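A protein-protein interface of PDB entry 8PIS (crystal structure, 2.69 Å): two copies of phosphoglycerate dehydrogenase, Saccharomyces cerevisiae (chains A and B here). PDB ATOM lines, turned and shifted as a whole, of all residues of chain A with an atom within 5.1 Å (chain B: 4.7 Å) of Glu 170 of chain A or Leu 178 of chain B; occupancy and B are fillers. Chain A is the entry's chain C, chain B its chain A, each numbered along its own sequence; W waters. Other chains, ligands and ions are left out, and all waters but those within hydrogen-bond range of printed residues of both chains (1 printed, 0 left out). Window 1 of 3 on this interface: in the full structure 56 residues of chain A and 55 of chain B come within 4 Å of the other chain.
Arg 176 of chain B touches Leu 166 of chain A.
CD1 of Leu 166 of chain A touches CD2 of Leu 178 of chain B, 3.5 Å away.
Glu 170 of chain A touches Leu 178 of chain B (OE2 to CD2, 3.7 Å).
Ile 347 of chain A touches Ser 182 of chain B (CA to OG, 3.8 Å).
CG2 of Thr 349 of chain A touches CD2 of Leu 178 of chain B, 3.7 Å away.
Of the printed residues of chain B, Leu 166 of chain A touches Arg 176 and Leu 178.
Glu 170 of chain A touches just one residue of chain B: Leu 178 (3.7 Å).
Ile 171 of chain A touches none of the printed residues of chain B.
Of the printed residues of chain B, Ile 347 of chain A touches Ser 182 (3.8 Å).
Of the printed residues of chain B, Ile 352 of chain A touches Arg 176 (2.8 Å).
Ser 173 of chain B touches none of the printed residues of chain A.
Of the printed residues of chain A, Arg 176 of chain B touches Leu 166 and Ile 352.
Leu 178 of chain B touches just these residues of chain A: Leu 166 (3.5 Å), Glu 170 (3.7 Å) and Thr 349 (3.7 Å).
Printed residues of chain A within 4 Å of Ser 182 of chain B: Ile 347 (3.8 Å).
The nearest printed residue of chain B that does not touch Glu 170 of chain A is Ser 173 of chain B (7.1 Å).
Water W1 bridges OE1 of Glu 165 of chain A and NH1 of Arg 176 of chain B.
Of the 16 printed residues of chain A, 5 touch a printed residue of chain B.
Among the printed residues, 6 pairs touch across the chains.
Among the printed residues, no Asp or Glu carboxylate lies within 4 Å of a Lys or Arg side-chain nitrogen of the other chain.
O of Ile 352 of chain A lies within hydrogen-bond range of NH2 of Arg 176 of chain B, at 2.8 Å.
O of Ser 173 of chain B lies within hydrogen-bond range of N of Leu 178 of chain B.
Position printed for both chains: 173.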
ATOM      1  N   GLU A 165      29.593 -14.732  -8.662  1.00  0.00           N
ATOM      2  CA  GLU A 165      29.264 -14.589  -7.247  1.00  0.00           C
ATOM      3  C   GLU A 165      27.874 -14.003  -7.082  1.00  0.00           C
ATOM      4  O   GLU A 165      27.111 -14.428  -6.207  1.00  0.00           O
ATOM      5  CB  GLU A 165      30.298 -13.726  -6.528  1.00  0.00           C
ATOM      6  CG  GLU A 165      31.685 -14.351  -6.465  1.00  0.00           C
ATOM      7  CD  GLU A 165      32.608 -13.615  -5.513  1.00  0.00           C
ATOM      8  OE1 GLU A 165      32.201 -12.558  -4.988  1.00  0.00           O
ATOM      9  OE2 GLU A 165      33.732 -14.104  -5.271  1.00  0.00           O
ATOM     10  N   LEU A 166      27.513 -13.056  -7.943  1.00  0.00           N
ATOM     11  CA  LEU A 166      26.169 -12.500  -7.914  1.00  0.00           C
ATOM     12  C   LEU A 166      25.123 -13.596  -8.009  1.00  0.00           C
ATOM     13  O   LEU A 166      24.189 -13.649  -7.205  1.00  0.00           O
ATOM     14  CB  LEU A 166      26.003 -11.510  -9.061  1.00  0.00           C
ATOM     15  CG  LEU A 166      24.585 -10.968  -9.192  1.00  0.00           C
ATOM     16  CD1 LEU A 166      24.212 -10.194  -7.937  1.00  0.00           C
ATOM     17  CD2 LEU A 166      24.458 -10.114 -10.453  1.00  0.00           C
ATOM     18  N   VAL A 167      25.291 -14.510  -8.961  1.00  0.00           N
ATOM     19  CA  VAL A 167      24.279 -15.534  -9.161  1.00  0.00           C
ATOM     20  C   VAL A 167      24.198 -16.451  -7.948  1.00  0.00           C
ATOM     21  O   VAL A 167      23.101 -16.755  -7.460  1.00  0.00           O
ATOM     22  CB  VAL A 167      24.568 -16.297 -10.469  1.00  0.00           C
ATOM     23  CG1 VAL A 167      23.567 -17.417 -10.689  1.00  0.00           C
ATOM     24  CG2 VAL A 167      24.525 -15.324 -11.654  1.00  0.00           C
ATOM     25  N   ILE A 168      25.349 -16.850  -7.393  1.00  0.00           N
ATOM     26  CA  ILE A 168      25.337 -17.684  -6.189  1.00  0.00           C
ATOM     27  C   ILE A 168      24.513 -17.008  -5.106  1.00  0.00           C
ATOM     28  O   ILE A 168      23.653 -17.627  -4.473  1.00  0.00           O
ATOM     29  CB  ILE A 168      26.772 -17.977  -5.709  1.00  0.00           C
ATOM     30  CG1 ILE A 168      27.509 -18.874  -6.704  1.00  0.00           C
ATOM     31  CG2 ILE A 168      26.770 -18.656  -4.344  1.00  0.00           C
ATOM     32  CD1 ILE A 168      26.890 -20.247  -6.846  1.00  0.00           C
ATOM     33  N   GLY A 169      24.750 -15.718  -4.890  1.00  0.00           N
ATOM     34  CA  GLY A 169      23.957 -15.004  -3.906  1.00  0.00           C
ATOM     35  C   GLY A 169      22.478 -14.991  -4.245  1.00  0.00           C
ATOM     36  O   GLY A 169      21.626 -15.090  -3.360  1.00  0.00           O
ATOM     37  N   GLU A 170      22.153 -14.881  -5.524  1.00  0.00           N
ATOM     38  CA  GLU A 170      20.752 -14.786  -5.898  1.00  0.00           C
ATOM     39  C   GLU A 170      20.079 -16.145  -5.944  1.00  0.00           C
ATOM     40  O   GLU A 170      18.868 -16.237  -5.711  1.00  0.00           O
ATOM     41  CB  GLU A 170      20.624 -14.044  -7.222  1.00  0.00           C
ATOM     42  CG  GLU A 170      20.997 -12.569  -7.050  1.00  0.00           C
ATOM     43  CD  GLU A 170      20.943 -11.774  -8.338  1.00  0.00           C
ATOM     44  OE1 GLU A 170      20.748 -12.378  -9.400  1.00  0.00           O
ATOM     45  OE2 GLU A 170      21.102 -10.536  -8.290  1.00  0.00           O
ATOM     46  N   ILE A 171      20.819 -17.207  -6.259  1.00  0.00           N
ATOM     47  CA  ILE A 171      20.250 -18.539  -6.091  1.00  0.00           C
ATOM     48  C   ILE A 171      19.801 -18.728  -4.652  1.00  0.00           C
ATOM     49  O   ILE A 171      18.671 -19.151  -4.383  1.00  0.00           O
ATOM     50  CB  ILE A 171      21.256 -19.625  -6.507  1.00  0.00           C
ATOM     51  CG1 ILE A 171      21.443 -19.654  -8.017  1.00  0.00           C
ATOM     52  CG2 ILE A 171      20.823 -20.987  -5.982  1.00  0.00           C
ATOM     53  CD1 ILE A 171      22.584 -20.536  -8.428  1.00  0.00           C
ATOM     54  N   ILE A 172      20.665 -18.362  -3.705  1.00  0.00           N
ATOM     55  CA  ILE A 172      20.338 -18.563  -2.301  1.00  0.00           C
ATOM     56  C   ILE A 172      19.209 -17.639  -1.871  1.00  0.00           C
ATOM     57  O   ILE A 172      18.304 -18.051  -1.133  1.00  0.00           O
ATOM     58  CB  ILE A 172      21.592 -18.394  -1.439  1.00  0.00           C
ATOM     59  CG1 ILE A 172      22.661 -19.383  -1.908  1.00  0.00           C
ATOM     60  CG2 ILE A 172      21.249 -18.691   0.004  1.00  0.00           C
ATOM     61  CD1 ILE A 172      24.036 -19.148  -1.322  1.00  0.00           C
ATOM     62  N   SER A 173      19.240 -16.379  -2.311  1.00  0.00           N
ATOM     63  CA  SER A 173      18.185 -15.450  -1.923  1.00  0.00           C
ATOM     64  C   SER A 173      16.836 -15.894  -2.454  1.00  0.00           C
ATOM     65  O   SER A 173      15.835 -15.855  -1.731  1.00  0.00           O
ATOM     66  CB  SER A 173      18.482 -14.041  -2.421  1.00  0.00           C
ATOM     67  OG  SER A 173      19.600 -13.502  -1.756  1.00  0.00           O
ATOM     68  N   LEU A 174      16.787 -16.325  -3.714  1.00  0.00           N
ATOM     69  CA  LEU A 174      15.518 -16.769  -4.273  1.00  0.00           C
ATOM     70  C   LEU A 174      15.040 -18.041  -3.588  1.00  0.00           C
ATOM     71  O   LEU A 174      13.872 -18.138  -3.199  1.00  0.00           O
ATOM     72  CB  LEU A 174      15.655 -16.963  -5.785  1.00  0.00           C
ATOM     73  CG  LEU A 174      15.794 -15.704  -6.659  1.00  0.00           C
ATOM     74  CD1 LEU A 174      16.099 -16.059  -8.099  1.00  0.00           C
ATOM     75  CD2 LEU A 174      14.516 -14.881  -6.603  1.00  0.00           C
ATOM     76  N   ALA A 175      15.950 -18.987  -3.351  1.00  0.00           N
ATOM     77  CA  ALA A 175      15.581 -20.227  -2.681  1.00  0.00           C
ATOM     78  C   ALA A 175      15.093 -20.000  -1.254  1.00  0.00           C
ATOM     79  O   ALA A 175      14.359 -20.840  -0.729  1.00  0.00           O
ATOM     80  CB  ALA A 175      16.767 -21.193  -2.673  1.00  0.00           C
ATOM     81  N   ILE A 287      17.272 -16.831 -13.456  1.00  0.00           N
ATOM     82  CA  ILE A 287      18.237 -15.778 -13.175  1.00  0.00           C
ATOM     83  C   ILE A 287      18.809 -15.321 -14.501  1.00  0.00           C
ATOM     84  O   ILE A 287      19.340 -16.139 -15.261  1.00  0.00           O
ATOM     85  CB  ILE A 287      19.346 -16.266 -12.239  1.00  0.00           C
ATOM     86  CG1 ILE A 287      18.714 -16.707 -10.923  1.00  0.00           C
ATOM     87  CG2 ILE A 287      20.391 -15.157 -12.013  1.00  0.00           C
ATOM     88  CD1 ILE A 287      19.672 -17.388  -9.989  1.00  0.00           C
ATOM     89  N   ALA A 313      15.528 -13.485 -10.796  1.00  0.00           N
ATOM     90  CA  ALA A 313      16.506 -12.443 -10.524  1.00  0.00           C
ATOM     91  C   ALA A 313      16.948 -11.861 -11.855  1.00  0.00           C
ATOM     92  O   ALA A 313      17.542 -12.568 -12.678  1.00  0.00           O
ATOM     93  CB  ALA A 313      17.697 -12.990  -9.740  1.00  0.00           C
ATOM     94  N   ILE A 347      14.144 -10.522  -7.629  1.00  0.00           N
ATOM     95  CA  ILE A 347      15.262  -9.650  -7.296  1.00  0.00           C
ATOM     96  C   ILE A 347      15.597  -8.846  -8.546  1.00  0.00           C
ATOM     97  O   ILE A 347      15.824  -9.419  -9.620  1.00  0.00           O
ATOM     98  CB  ILE A 347      16.487 -10.445  -6.812  1.00  0.00           C
ATOM     99  CG1 ILE A 347      16.159 -11.305  -5.606  1.00  0.00           C
ATOM    100  CG2 ILE A 347      17.607  -9.491  -6.418  1.00  0.00           C
ATOM    101  CD1 ILE A 347      17.264 -12.306  -5.288  1.00  0.00           C
ATOM    102  N   THR A 349      18.125  -5.859 -10.126  1.00  0.00           N
ATOM    103  CA  THR A 349      19.348  -5.118  -9.884  1.00  0.00           C
ATOM    104  C   THR A 349      19.702  -4.242 -11.076  1.00  0.00           C
ATOM    105  O   THR A 349      19.523  -4.643 -12.229  1.00  0.00           O
ATOM    106  CB  THR A 349      20.523  -6.057  -9.579  1.00  0.00           C
ATOM    107  OG1 THR A 349      20.654  -7.038 -10.622  1.00  0.00           O
ATOM    108  CG2 THR A 349      20.352  -6.704  -8.199  1.00  0.00           C
ATOM    109  N   ILE A 352      24.219  -4.524 -12.178  1.00  0.00           N
ATOM    110  CA  ILE A 352      25.389  -4.464 -11.315  1.00  0.00           C
ATOM    111  C   ILE A 352      26.229  -5.733 -11.408  1.00  0.00           C
ATOM    112  O   ILE A 352      27.170  -5.902 -10.623  1.00  0.00           O
ATOM    113  CB  ILE A 352      24.983  -4.160  -9.862  1.00  0.00           C
ATOM    114  CG1 ILE A 352      23.939  -5.152  -9.344  1.00  0.00           C
ATOM    115  CG2 ILE A 352      24.408  -2.766  -9.759  1.00  0.00           C
ATOM    116  CD1 ILE A 352      24.501  -6.399  -8.717  1.00  0.00           C
ATOM    117  N   SER B 173      25.133 -10.888  -0.458  1.00  0.00           N
ATOM    118  CA  SER B 173      24.157  -9.806  -0.585  1.00  0.00           C
ATOM    119  C   SER B 173      24.682  -8.515   0.025  1.00  0.00           C
ATOM    120  O   SER B 173      24.552  -7.441  -0.574  1.00  0.00           O
ATOM    121  CB  SER B 173      22.834 -10.201   0.069  1.00  0.00           C
ATOM    122  N   ARG B 176      27.472  -6.953  -2.054  1.00  0.00           N
ATOM    123  CA  ARG B 176      27.030  -6.412  -3.328  1.00  0.00           C
ATOM    124  C   ARG B 176      25.866  -5.452  -3.159  1.00  0.00           C
ATOM    125  O   ARG B 176      25.368  -4.916  -4.153  1.00  0.00           O
ATOM    126  CB  ARG B 176      26.640  -7.550  -4.273  1.00  0.00           C
ATOM    127  CG  ARG B 176      27.783  -8.502  -4.530  1.00  0.00           C
ATOM    128  CD  ARG B 176      28.840  -7.821  -5.343  1.00  0.00           C
ATOM    129  NE  ARG B 176      28.324  -7.494  -6.668  1.00  0.00           N
ATOM    130  CZ  ARG B 176      28.365  -8.341  -7.689  1.00  0.00           C
ATOM    131  NH1 ARG B 176      28.911  -9.545  -7.535  1.00  0.00           N
ATOM    132  NH2 ARG B 176      27.876  -7.985  -8.864  1.00  0.00           N
ATOM    133  N   GLN B 177      25.395  -5.267  -1.930  1.00  0.00           N
ATOM    134  CA  GLN B 177      24.288  -4.367  -1.631  1.00  0.00           C
ATOM    135  C   GLN B 177      23.031  -4.744  -2.423  1.00  0.00           C
ATOM    136  O   GLN B 177      22.298  -3.881  -2.899  1.00  0.00           O
ATOM    137  CB  GLN B 177      24.700  -2.915  -1.883  1.00  0.00           C
ATOM    138  CG  GLN B 177      25.876  -2.458  -1.000  1.00  0.00           C
ATOM    139  CD  GLN B 177      26.288  -1.014  -1.260  1.00  0.00           C
ATOM    140  OE1 GLN B 177      25.708  -0.340  -2.105  1.00  0.00           O
ATOM    141  NE2 GLN B 177      27.309  -0.551  -0.563  1.00  0.00           N
ATOM    142  N   LEU B 178      22.762  -6.053  -2.527  1.00  0.00           N
ATOM    143  CA  LEU B 178      21.605  -6.530  -3.285  1.00  0.00           C
ATOM    144  C   LEU B 178      20.285  -6.037  -2.704  1.00  0.00           C
ATOM    145  O   LEU B 178      19.374  -5.651  -3.450  1.00  0.00           O
ATOM    146  CB  LEU B 178      21.595  -8.055  -3.350  1.00  0.00           C
ATOM    147  CG  LEU B 178      22.645  -8.737  -4.203  1.00  0.00           C
ATOM    148  CD1 LEU B 178      22.515 -10.243  -4.041  1.00  0.00           C
ATOM    149  CD2 LEU B 178      22.406  -8.318  -5.625  1.00  0.00           C
ATOM    150  N   GLY B 179      20.128  -6.123  -1.383  1.00  0.00           N
ATOM    151  CA  GLY B 179      18.892  -5.662  -0.766  1.00  0.00           C
ATOM    152  C   GLY B 179      18.531  -4.240  -1.150  1.00  0.00           C
ATOM    153  O   GLY B 179      17.408  -3.961  -1.577  1.00  0.00           O
ATOM    154  N   ASP B 180      19.486  -3.316  -1.015  1.00  0.00           N
ATOM    155  CA  ASP B 180      19.195  -1.918  -1.313  1.00  0.00           C
ATOM    156  C   ASP B 180      18.910  -1.720  -2.794  1.00  0.00           C
ATOM    157  O   ASP B 180      17.909  -1.092  -3.163  1.00  0.00           O
ATOM    158  CB  ASP B 180      20.341  -1.024  -0.852  1.00  0.00           C
ATOM    159  CG  ASP B 180      20.442  -0.948   0.658  1.00  0.00           C
ATOM    160  OD1 ASP B 180      19.412  -1.110   1.344  1.00  0.00           O
ATOM    161  OD2 ASP B 180      21.554  -0.704   1.157  1.00  0.00           O
ATOM    162  N   ARG B 181      19.775  -2.249  -3.658  1.00  0.00           N
ATOM    163  CA  ARG B 181      19.562  -2.084  -5.088  1.00  0.00           C
ATOM    164  C   ARG B 181      18.164  -2.539  -5.490  1.00  0.00           C
ATOM    165  O   ARG B 181      17.463  -1.835  -6.225  1.00  0.00           O
ATOM    166  CB  ARG B 181      20.615  -2.868  -5.866  1.00  0.00           C
ATOM    167  CG  ARG B 181      22.060  -2.495  -5.577  1.00  0.00           C
ATOM    168  CD  ARG B 181      22.439  -1.164  -6.172  1.00  0.00           C
ATOM    169  NE  ARG B 181      21.948  -0.047  -5.375  1.00  0.00           N
ATOM    170  CZ  ARG B 181      22.538   0.383  -4.266  1.00  0.00           C
ATOM    171  NH1 ARG B 181      23.651  -0.204  -3.838  1.00  0.00           N
ATOM    172  NH2 ARG B 181      22.027   1.407  -3.598  1.00  0.00           N
ATOM    173  N   SER B 182      17.717  -3.686  -4.966  1.00  0.00           N
ATOM    174  CA  SER B 182      16.442  -4.253  -5.401  1.00  0.00           C
ATOM    175  C   SER B 182      15.253  -3.501  -4.819  1.00  0.00           C
ATOM    176  O   SER B 182      14.211  -3.376  -5.474  1.00  0.00           O
ATOM    177  CB  SER B 182      16.358  -5.731  -5.039  1.00  0.00           C
ATOM    178  OG  SER B 182      15.121  -6.252  -5.492  1.00  0.00           O
HETATM  179  O   HOH W   1      30.145 -10.803  -4.900  1.00  0.00           O
